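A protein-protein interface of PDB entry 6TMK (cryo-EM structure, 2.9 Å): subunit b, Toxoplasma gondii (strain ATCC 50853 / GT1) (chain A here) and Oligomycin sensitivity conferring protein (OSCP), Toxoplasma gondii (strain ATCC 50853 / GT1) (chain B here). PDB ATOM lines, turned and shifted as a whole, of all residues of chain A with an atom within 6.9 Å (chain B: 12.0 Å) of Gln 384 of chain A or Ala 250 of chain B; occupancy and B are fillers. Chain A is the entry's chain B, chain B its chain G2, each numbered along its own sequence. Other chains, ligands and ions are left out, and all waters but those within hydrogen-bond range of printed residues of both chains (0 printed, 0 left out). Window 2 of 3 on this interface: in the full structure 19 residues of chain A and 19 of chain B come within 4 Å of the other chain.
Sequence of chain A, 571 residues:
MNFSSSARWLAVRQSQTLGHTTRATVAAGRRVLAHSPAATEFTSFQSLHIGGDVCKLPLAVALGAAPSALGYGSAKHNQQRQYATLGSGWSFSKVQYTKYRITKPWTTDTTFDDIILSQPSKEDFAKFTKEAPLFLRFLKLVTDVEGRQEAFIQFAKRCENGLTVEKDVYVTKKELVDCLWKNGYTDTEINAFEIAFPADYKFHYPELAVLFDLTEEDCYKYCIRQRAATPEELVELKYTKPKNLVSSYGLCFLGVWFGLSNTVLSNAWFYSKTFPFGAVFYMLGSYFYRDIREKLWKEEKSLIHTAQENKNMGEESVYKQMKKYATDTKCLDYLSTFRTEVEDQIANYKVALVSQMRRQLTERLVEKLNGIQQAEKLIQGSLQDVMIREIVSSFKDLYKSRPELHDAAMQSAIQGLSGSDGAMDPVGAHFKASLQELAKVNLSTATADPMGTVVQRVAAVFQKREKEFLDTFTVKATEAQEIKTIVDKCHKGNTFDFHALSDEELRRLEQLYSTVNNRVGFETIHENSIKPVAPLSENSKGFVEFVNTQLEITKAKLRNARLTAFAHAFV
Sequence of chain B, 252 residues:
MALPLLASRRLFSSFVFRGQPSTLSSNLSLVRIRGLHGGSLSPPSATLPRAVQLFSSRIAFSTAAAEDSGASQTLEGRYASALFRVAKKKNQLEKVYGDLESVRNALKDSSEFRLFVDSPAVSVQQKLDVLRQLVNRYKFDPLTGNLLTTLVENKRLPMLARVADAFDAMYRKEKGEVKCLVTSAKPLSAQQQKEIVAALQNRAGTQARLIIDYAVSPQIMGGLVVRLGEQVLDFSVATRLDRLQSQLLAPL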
ATOM      1  N   LYS A 377     -12.706  12.905   4.790  1.00  0.00           N
ATOM      2  CA  LYS A 377     -13.105  11.785   3.944  1.00  0.00           C
ATOM      3  C   LYS A 377     -13.632  12.280   2.604  1.00  0.00           C
ATOM      4  O   LYS A 377     -13.243  11.775   1.544  1.00  0.00           O
ATOM      5  CB  LYS A 377     -14.158  10.939   4.658  1.00  0.00           C
ATOM      6  CG  LYS A 377     -14.204   9.496   4.187  1.00  0.00           C
ATOM      7  CD  LYS A 377     -14.941   8.615   5.177  1.00  0.00           C
ATOM      8  CE  LYS A 377     -14.025   8.167   6.303  1.00  0.00           C
ATOM      9  NZ  LYS A 377     -13.252   6.948   5.941  1.00  0.00           N
ATOM     10  N   ILE A 379     -13.073  15.093   1.199  1.00  0.00           N
ATOM     11  CA  ILE A 379     -11.953  15.698   0.485  1.00  0.00           C
ATOM     12  C   ILE A 379     -11.212  14.637  -0.315  1.00  0.00           C
ATOM     13  O   ILE A 379     -10.993  14.786  -1.522  1.00  0.00           O
ATOM     14  CB  ILE A 379     -11.016  16.415   1.475  1.00  0.00           C
ATOM     15  CG1 ILE A 379     -11.550  17.814   1.790  1.00  0.00           C
ATOM     16  CG2 ILE A 379      -9.594  16.495   0.910  1.00  0.00           C
ATOM     17  CD1 ILE A 379     -10.827  18.512   2.926  1.00  0.00           C
ATOM     18  N   GLN A 380     -10.813  13.550   0.349  1.00  0.00           N
ATOM     19  CA  GLN A 380     -10.010  12.541  -0.338  1.00  0.00           C
ATOM     20  C   GLN A 380     -10.828  11.827  -1.411  1.00  0.00           C
ATOM     21  O   GLN A 380     -10.300  11.480  -2.479  1.00  0.00           O
ATOM     22  CB  GLN A 380      -9.438  11.545   0.673  1.00  0.00           C
ATOM     23  CG  GLN A 380     -10.342  10.365   1.007  1.00  0.00           C
ATOM     24  CD  GLN A 380      -9.708   9.415   2.002  1.00  0.00           C
ATOM     25  OE1 GLN A 380      -8.637   9.686   2.541  1.00  0.00           O
ATOM     26  NE2 GLN A 380     -10.369   8.291   2.250  1.00  0.00           N
ATOM     27  N   GLY A 381     -12.119  11.620  -1.156  1.00  0.00           N
ATOM     28  CA  GLY A 381     -13.016  11.084  -2.159  1.00  0.00           C
ATOM     29  C   GLY A 381     -13.051  11.915  -3.424  1.00  0.00           C
ATOM     30  O   GLY A 381     -12.788  11.403  -4.520  1.00  0.00           O
ATOM     31  N   SER A 382     -13.389  13.202  -3.288  1.00  0.00           N
ATOM     32  CA  SER A 382     -13.405  14.083  -4.450  1.00  0.00           C
ATOM     33  C   SER A 382     -12.036  14.154  -5.114  1.00  0.00           C
ATOM     34  O   SER A 382     -11.945  14.247  -6.346  1.00  0.00           O
ATOM     35  CB  SER A 382     -13.867  15.482  -4.042  1.00  0.00           C
ATOM     36  OG  SER A 382     -13.966  16.332  -5.170  1.00  0.00           O
ATOM     37  N   LEU A 383     -10.964  14.081  -4.322  1.00  0.00           N
ATOM     38  CA  LEU A 383      -9.622  14.155  -4.883  1.00  0.00           C
ATOM     39  C   LEU A 383      -9.370  12.989  -5.828  1.00  0.00           C
ATOM     40  O   LEU A 383      -8.978  13.187  -6.983  1.00  0.00           O
ATOM     41  CB  LEU A 383      -8.587  14.175  -3.756  1.00  0.00           C
ATOM     42  CG  LEU A 383      -7.126  14.388  -4.160  1.00  0.00           C
ATOM     43  CD1 LEU A 383      -6.383  15.130  -3.062  1.00  0.00           C
ATOM     44  CD2 LEU A 383      -6.435  13.063  -4.463  1.00  0.00           C
ATOM     45  N   GLN A 384      -9.572  11.760  -5.347  1.00  0.00           N
ATOM     46  CA  GLN A 384      -9.332  10.607  -6.210  1.00  0.00           C
ATOM     47  C   GLN A 384     -10.310  10.574  -7.378  1.00  0.00           C
ATOM     48  O   GLN A 384      -9.938  10.177  -8.492  1.00  0.00           O
ATOM     49  CB  GLN A 384      -9.425   9.309  -5.408  1.00  0.00           C
ATOM     50  CG  GLN A 384     -10.786   9.056  -4.784  1.00  0.00           C
ATOM     51  CD  GLN A 384     -10.784   7.866  -3.847  1.00  0.00           C
ATOM     52  OE1 GLN A 384      -9.750   7.239  -3.623  1.00  0.00           O
ATOM     53  NE2 GLN A 384     -11.948   7.548  -3.292  1.00  0.00           N
ATOM     54  N   ASP A 385     -11.553  11.014  -7.154  1.00  0.00           N
ATOM     55  CA  ASP A 385     -12.514  11.137  -8.244  1.00  0.00           C
ATOM     56  C   ASP A 385     -11.960  11.986  -9.383  1.00  0.00           C
ATOM     57  O   ASP A 385     -11.931  11.552 -10.543  1.00  0.00           O
ATOM     58  CB  ASP A 385     -13.820  11.734  -7.719  1.00  0.00           C
ATOM     59  CG  ASP A 385     -14.790  12.081  -8.832  1.00  0.00           C
ATOM     60  OD1 ASP A 385     -15.487  11.166  -9.322  1.00  0.00           O
ATOM     61  OD2 ASP A 385     -14.856  13.267  -9.220  1.00  0.00           O
ATOM     62  N   VAL A 386     -11.514  13.205  -9.071  1.00  0.00           N
ATOM     63  CA  VAL A 386     -11.013  14.067 -10.135  1.00  0.00           C
ATOM     64  C   VAL A 386      -9.701  13.531 -10.694  1.00  0.00           C
ATOM     65  O   VAL A 386      -9.425  13.687 -11.888  1.00  0.00           O
ATOM     66  CB  VAL A 386     -10.852  15.517  -9.636  1.00  0.00           C
ATOM     67  CG1 VAL A 386      -9.920  15.582  -8.430  1.00  0.00           C
ATOM     68  CG2 VAL A 386     -10.345  16.412 -10.758  1.00  0.00           C
ATOM     69  N   MET A 387      -8.868  12.908  -9.857  1.00  0.00           N
ATOM     70  CA  MET A 387      -7.609  12.363 -10.356  1.00  0.00           C
ATOM     71  C   MET A 387      -7.860  11.303 -11.421  1.00  0.00           C
ATOM     72  O   MET A 387      -7.197  11.291 -12.470  1.00  0.00           O
ATOM     73  CB  MET A 387      -6.803  11.779  -9.196  1.00  0.00           C
ATOM     74  CG  MET A 387      -5.329  11.585  -9.496  1.00  0.00           C
ATOM     75  SD  MET A 387      -4.604  10.238  -8.543  1.00  0.00           S
ATOM     76  CE  MET A 387      -4.442  11.013  -6.937  1.00  0.00           C
ATOM     77  N   ILE A 388      -8.934  10.532 -11.254  1.00  0.00           N
ATOM     78  CA  ILE A 388      -9.273   9.525 -12.252  1.00  0.00           C
ATOM     79  C   ILE A 388      -9.904  10.185 -13.463  1.00  0.00           C
ATOM     80  O   ILE A 388      -9.567   9.853 -14.607  1.00  0.00           O
ATOM     81  CB  ILE A 388     -10.199   8.459 -11.639  1.00  0.00           C
ATOM     82  CG1 ILE A 388      -9.467   7.651 -10.562  1.00  0.00           C
ATOM     83  CG2 ILE A 388     -10.733   7.530 -12.723  1.00  0.00           C
ATOM     84  CD1 ILE A 388      -8.207   6.953 -11.040  1.00  0.00           C
ATOM     85  N   ARG A 389     -10.836  11.114 -13.245  1.00  0.00           N
ATOM     86  CA  ARG A 389     -11.491  11.748 -14.380  1.00  0.00           C
ATOM     87  C   ARG A 389     -10.441  12.374 -15.288  1.00  0.00           C
ATOM     88  O   ARG A 389     -10.492  12.228 -16.517  1.00  0.00           O
ATOM     89  CB  ARG A 389     -12.495  12.794 -13.899  1.00  0.00           C
ATOM     90  CG  ARG A 389     -13.655  12.205 -13.120  1.00  0.00           C
ATOM     91  CD  ARG A 389     -14.796  11.815 -14.041  1.00  0.00           C
ATOM     92  NE  ARG A 389     -15.903  11.207 -13.309  1.00  0.00           N
ATOM     93  CZ  ARG A 389     -15.878   9.976 -12.806  1.00  0.00           C
ATOM     94  NH1 ARG A 389     -14.800   9.217 -12.947  1.00  0.00           N
ATOM     95  NH2 ARG A 389     -16.932   9.506 -12.155  1.00  0.00           N
ATOM     96  N   GLU A 390      -9.466  13.063 -14.689  1.00  0.00           N
ATOM     97  CA  GLU A 390      -8.496  13.815 -15.468  1.00  0.00           C
ATOM     98  C   GLU A 390      -7.489  12.885 -16.131  1.00  0.00           C
ATOM     99  O   GLU A 390      -7.096  13.121 -17.276  1.00  0.00           O
ATOM    100  CB  GLU A 390      -7.785  14.836 -14.582  1.00  0.00           C
ATOM    101  CG  GLU A 390      -6.791  15.717 -15.327  1.00  0.00           C
ATOM    102  CD  GLU A 390      -7.426  16.475 -16.476  1.00  0.00           C
ATOM    103  OE1 GLU A 390      -8.634  16.784 -16.393  1.00  0.00           O
ATOM    104  OE2 GLU A 390      -6.718  16.759 -17.467  1.00  0.00           O
ATOM    105  N   VAL A 458      -5.336  18.970 -10.845  1.00  0.00           N
ATOM    106  CA  VAL A 458      -5.851  18.332  -9.641  1.00  0.00           C
ATOM    107  C   VAL A 458      -5.469  19.148  -8.413  1.00  0.00           C
ATOM    108  O   VAL A 458      -6.222  19.197  -7.432  1.00  0.00           O
ATOM    109  CB  VAL A 458      -5.340  16.884  -9.524  1.00  0.00           C
ATOM    110  CG1 VAL A 458      -3.875  16.861  -9.111  1.00  0.00           C
ATOM    111  CG2 VAL A 458      -6.188  16.103  -8.537  1.00  0.00           C
ATOM    112  N   LEU B 241     -10.224   0.453 -20.508  1.00  0.00           N
ATOM    113  CA  LEU B 241     -10.145   1.777 -19.898  1.00  0.00           C
ATOM    114  C   LEU B 241     -11.290   1.994 -18.916  1.00  0.00           C
ATOM    115  O   LEU B 241     -11.071   2.398 -17.766  1.00  0.00           O
ATOM    116  CB  LEU B 241     -10.146   2.851 -20.987  1.00  0.00           C
ATOM    117  CG  LEU B 241     -10.047   4.306 -20.522  1.00  0.00           C
ATOM    118  CD1 LEU B 241      -9.216   5.115 -21.505  1.00  0.00           C
ATOM    119  CD2 LEU B 241     -11.427   4.928 -20.355  1.00  0.00           C
ATOM    120  N   ASP B 242     -12.526   1.755 -19.356  1.00  0.00           N
ATOM    121  CA  ASP B 242     -13.679   2.015 -18.503  1.00  0.00           C
ATOM    122  C   ASP B 242     -13.707   1.057 -17.319  1.00  0.00           C
ATOM    123  O   ASP B 242     -14.061   1.455 -16.202  1.00  0.00           O
ATOM    124  CB  ASP B 242     -14.970   1.904 -19.313  1.00  0.00           C
ATOM    125  CG  ASP B 242     -16.201   1.784 -18.436  1.00  0.00           C
ATOM    126  OD1 ASP B 242     -16.772   2.831 -18.066  1.00  0.00           O
ATOM    127  OD2 ASP B 242     -16.595   0.643 -18.115  1.00  0.00           O
ATOM    128  N   ARG B 243     -13.362  -0.215 -17.542  1.00  0.00           N
ATOM    129  CA  ARG B 243     -13.289  -1.157 -16.431  1.00  0.00           C
ATOM    130  C   ARG B 243     -12.267  -0.691 -15.400  1.00  0.00           C
ATOM    131  O   ARG B 243     -12.529  -0.727 -14.192  1.00  0.00           O
ATOM    132  CB  ARG B 243     -12.931  -2.547 -16.953  1.00  0.00           C
ATOM    133  CG  ARG B 243     -13.344  -3.686 -16.041  1.00  0.00           C
ATOM    134  CD  ARG B 243     -13.523  -4.968 -16.834  1.00  0.00           C
ATOM    135  NE  ARG B 243     -12.452  -5.149 -17.814  1.00  0.00           N
ATOM    136  CZ  ARG B 243     -12.593  -5.023 -19.133  1.00  0.00           C
ATOM    137  NH1 ARG B 243     -11.548  -5.215 -19.926  1.00  0.00           N
ATOM    138  NH2 ARG B 243     -13.762  -4.698 -19.670  1.00  0.00           N
ATOM    139  N   LEU B 244     -11.107  -0.224 -15.862  1.00  0.00           N
ATOM    140  CA  LEU B 244     -10.079   0.263 -14.950  1.00  0.00           C
ATOM    141  C   LEU B 244     -10.591   1.462 -14.165  1.00  0.00           C
ATOM    142  O   LEU B 244     -10.366   1.570 -12.955  1.00  0.00           O
ATOM    143  CB  LEU B 244      -8.819   0.621 -15.740  1.00  0.00           C
ATOM    144  CG  LEU B 244      -7.528   0.817 -14.946  1.00  0.00           C
ATOM    145  CD1 LEU B 244      -7.046  -0.498 -14.357  1.00  0.00           C
ATOM    146  CD2 LEU B 244      -6.457   1.426 -15.837  1.00  0.00           C
ATOM    147  N   GLN B 245     -11.218   2.413 -14.859  1.00  0.00           N
ATOM    148  CA  GLN B 245     -11.755   3.595 -14.193  1.00  0.00           C
ATOM    149  C   GLN B 245     -12.754   3.202 -13.107  1.00  0.00           C
ATOM    150  O   GLN B 245     -12.670   3.672 -11.965  1.00  0.00           O
ATOM    151  CB  GLN B 245     -12.411   4.517 -15.224  1.00  0.00           C
ATOM    152  CG  GLN B 245     -13.494   5.423 -14.661  1.00  0.00           C
ATOM    153  CD  GLN B 245     -13.897   6.515 -15.630  1.00  0.00           C
ATOM    154  OE1 GLN B 245     -13.364   6.608 -16.736  1.00  0.00           O
ATOM    155  NE2 GLN B 245     -14.845   7.349 -15.222  1.00  0.00           N
ATOM    156  N   SER B 246     -13.745   2.382 -13.468  1.00  0.00           N
ATOM    157  CA  SER B 246     -14.734   1.925 -12.497  1.00  0.00           C
ATOM    158  C   SER B 246     -14.108   1.110 -11.375  1.00  0.00           C
ATOM    159  O   SER B 246     -14.698   1.007 -10.294  1.00  0.00           O
ATOM    160  CB  SER B 246     -15.809   1.096 -13.201  1.00  0.00           C
ATOM    161  OG  SER B 246     -16.526   1.880 -14.138  1.00  0.00           O
ATOM    162  N   GLN B 247     -12.928   0.530 -11.604  1.00  0.00           N
ATOM    163  CA  GLN B 247     -12.224  -0.159 -10.528  1.00  0.00           C
ATOM    164  C   GLN B 247     -11.567   0.841  -9.585  1.00  0.00           C
ATOM    165  O   GLN B 247     -11.664   0.711  -8.361  1.00  0.00           O
ATOM    166  CB  GLN B 247     -11.181  -1.112 -11.113  1.00  0.00           C
ATOM    167  CG  GLN B 247     -10.488  -1.983 -10.082  1.00  0.00           C
ATOM    168  CD  GLN B 247      -9.484  -2.932 -10.704  1.00  0.00           C
ATOM    169  OE1 GLN B 247      -8.302  -2.917 -10.359  1.00  0.00           O
ATOM    170  NE2 GLN B 247      -9.950  -3.765 -11.627  1.00  0.00           N
ATOM    171  N   LEU B 248     -10.896   1.843 -10.145  1.00  0.00           N
ATOM    172  CA  LEU B 248     -10.106   2.785  -9.367  1.00  0.00           C
ATOM    173  C   LEU B 248     -10.938   3.936  -8.822  1.00  0.00           C
ATOM    174  O   LEU B 248     -10.384   4.832  -8.178  1.00  0.00           O
ATOM    175  CB  LEU B 248      -8.957   3.346 -10.211  1.00  0.00           C
ATOM    176  CG  LEU B 248      -8.039   2.315 -10.863  1.00  0.00           C
ATOM    177  CD1 LEU B 248      -7.259   2.947 -12.003  1.00  0.00           C
ATOM    178  CD2 LEU B 248      -7.102   1.713  -9.831  1.00  0.00           C
ATOM    179  N   LEU B 249     -12.247   3.935  -9.065  1.00  0.00           N
ATOM    180  CA  LEU B 249     -13.141   4.775  -8.276  1.00  0.00           C
ATOM    181  C   LEU B 249     -13.529   4.121  -6.956  1.00  0.00           C
ATOM    182  O   LEU B 249     -14.357   4.674  -6.224  1.00  0.00           O
ATOM    183  CB  LEU B 249     -14.410   5.111  -9.068  1.00  0.00           C
ATOM    184  CG  LEU B 249     -14.271   5.922 -10.358  1.00  0.00           C
ATOM    185  CD1 LEU B 249     -15.649   6.243 -10.915  1.00  0.00           C
ATOM    186  CD2 LEU B 249     -13.475   7.199 -10.130  1.00  0.00           C
ATOM    187  N   ALA B 250     -12.951   2.960  -6.643  1.00  0.00           N
ATOM    188  CA  ALA B 250     -13.252   2.276  -5.400  1.00  0.00           C
ATOM    189  C   ALA B 250     -12.874   3.164  -4.215  1.00  0.00           C
ATOM    190  O   ALA B 250     -12.089   4.105  -4.359  1.00  0.00           O
ATOM    191  CB  ALA B 250     -12.503   0.947  -5.330  1.00  0.00           C
ATOM    192  N   PRO B 251     -13.417   2.884  -3.028  1.00  0.00           N
ATOM    193  CA  PRO B 251     -13.089   3.706  -1.856  1.00  0.00           C
ATOM    194  C   PRO B 251     -11.786   3.235  -1.224  1.00  0.00           C
ATOM    195  O   PRO B 251     -11.688   2.100  -0.752  1.00  0.00           O
ATOM    196  CB  PRO B 251     -14.284   3.479  -0.924  1.00  0.00           C
ATOM    197  CG  PRO B 251     -14.701   2.074  -1.227  1.00  0.00           C
ATOM    198  CD  PRO B 251     -14.415   1.847  -2.703  1.00  0.00           C
ATOM    199  N   LEU B 252     -10.787   4.112  -1.216  1.00  0.00           N
ATOM    200  CA  LEU B 252      -9.510   3.829  -0.569  1.00  0.00           C
ATOM    201  C   LEU B 252      -8.873   2.570  -1.149  1.00  0.00           C
ATOM    202  O   LEU B 252      -9.075   1.468  -0.639  1.00  0.00           O
ATOM    203  CB  LEU B 252      -9.689   3.678   0.944  1.00  0.00           C
ATOM    204  CG  LEU B 252      -9.799   4.993   1.719  1.00  0.00           C
ATOM    205  CD1 LEU B 252     -10.729   4.838   2.911  1.00  0.00           C
ATOM    206  CD2 LEU B 252      -8.424   5.468   2.164  1.00  0.00           C
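Hydrophobic or aromatic side chains of chain B that line the printed part of chain A: Leu 248, Leu 249 and Leu 252. Hydrophobic or aromatic side chains of chain A within 4 Å of the printed part of chain B: Ile 388. Among the printed residues, 7 pairs touch across the chains. Among the printed residues, no Asp or Glu carboxylate lies within 4 Å of a Lys or Arg side-chain nitrogen of the other chain.
The guanidinium group of Arg 389 of chain A sits close to the side-chain amide nitrogen of Gln 245 of chain B, 2.9 Å away.
The side-chain carboxylate (OD1) of Asp 385 of chain A lies within salt-bridge range of the guanidinium group (NH2) of Arg 389 of chain A (3.6 Å).
Gln 380 of chain A touches just one residue of chain B: Leu 252. No residue of chain B comes within 4 Å of Gly 381 of chain A. No residue of chain B comes within 4 Å of Ser 382 of chain A. Gln 384 of chain A touches one residue of chain B. No residue of chain B comes within 4 Å of Asp 385 of chain A. No residue of chain B comes within 4 Å of Val 386 of chain A. Met 387 of chain A touches none of the printed residues of chain B. Printed residues of chain B within 4 Å of Ile 388 of chain A: Gln 245, Leu 248 and Leu 249. Printed residues of chain A within 4 Å of Gln 245 of chain B: Ile 388 and Arg 389. Gln 247 of chain B touches none of the printed residues of chain A. Ala 250 of chain B touches just one residue of chain A: Gln 384. Printed residues of chain A within 4 Å of Leu 252 of chain B: Gln 380 (3.4 Å). The nearest printed residue of chain A that does not touch Ala 250 of chain B is Ile 388 of chain A (7.0 Å). The nearest printed residue of chain A that does not touch Leu 248 of chain B is Gln 384 of chain A (5.2 Å).
CG of Leu 252 of chain B touches NE2 of Gln 380 of chain A, 3.4 Å away. Gln 384 of chain A touches Ala 250 of chain B (NE2 to O, 3.6 Å). Gln 245 of chain B touches Ile 388 of chain A. Ile 388 of chain A touches Leu 248 of chain B. Ile 388 of chain A touches Leu 249 of chain B (CG2 to CD2, 3.8 Å). CD1 of Leu 249 of chain B touches NH1 of Arg 389 of chain A, at 3.7 Å.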
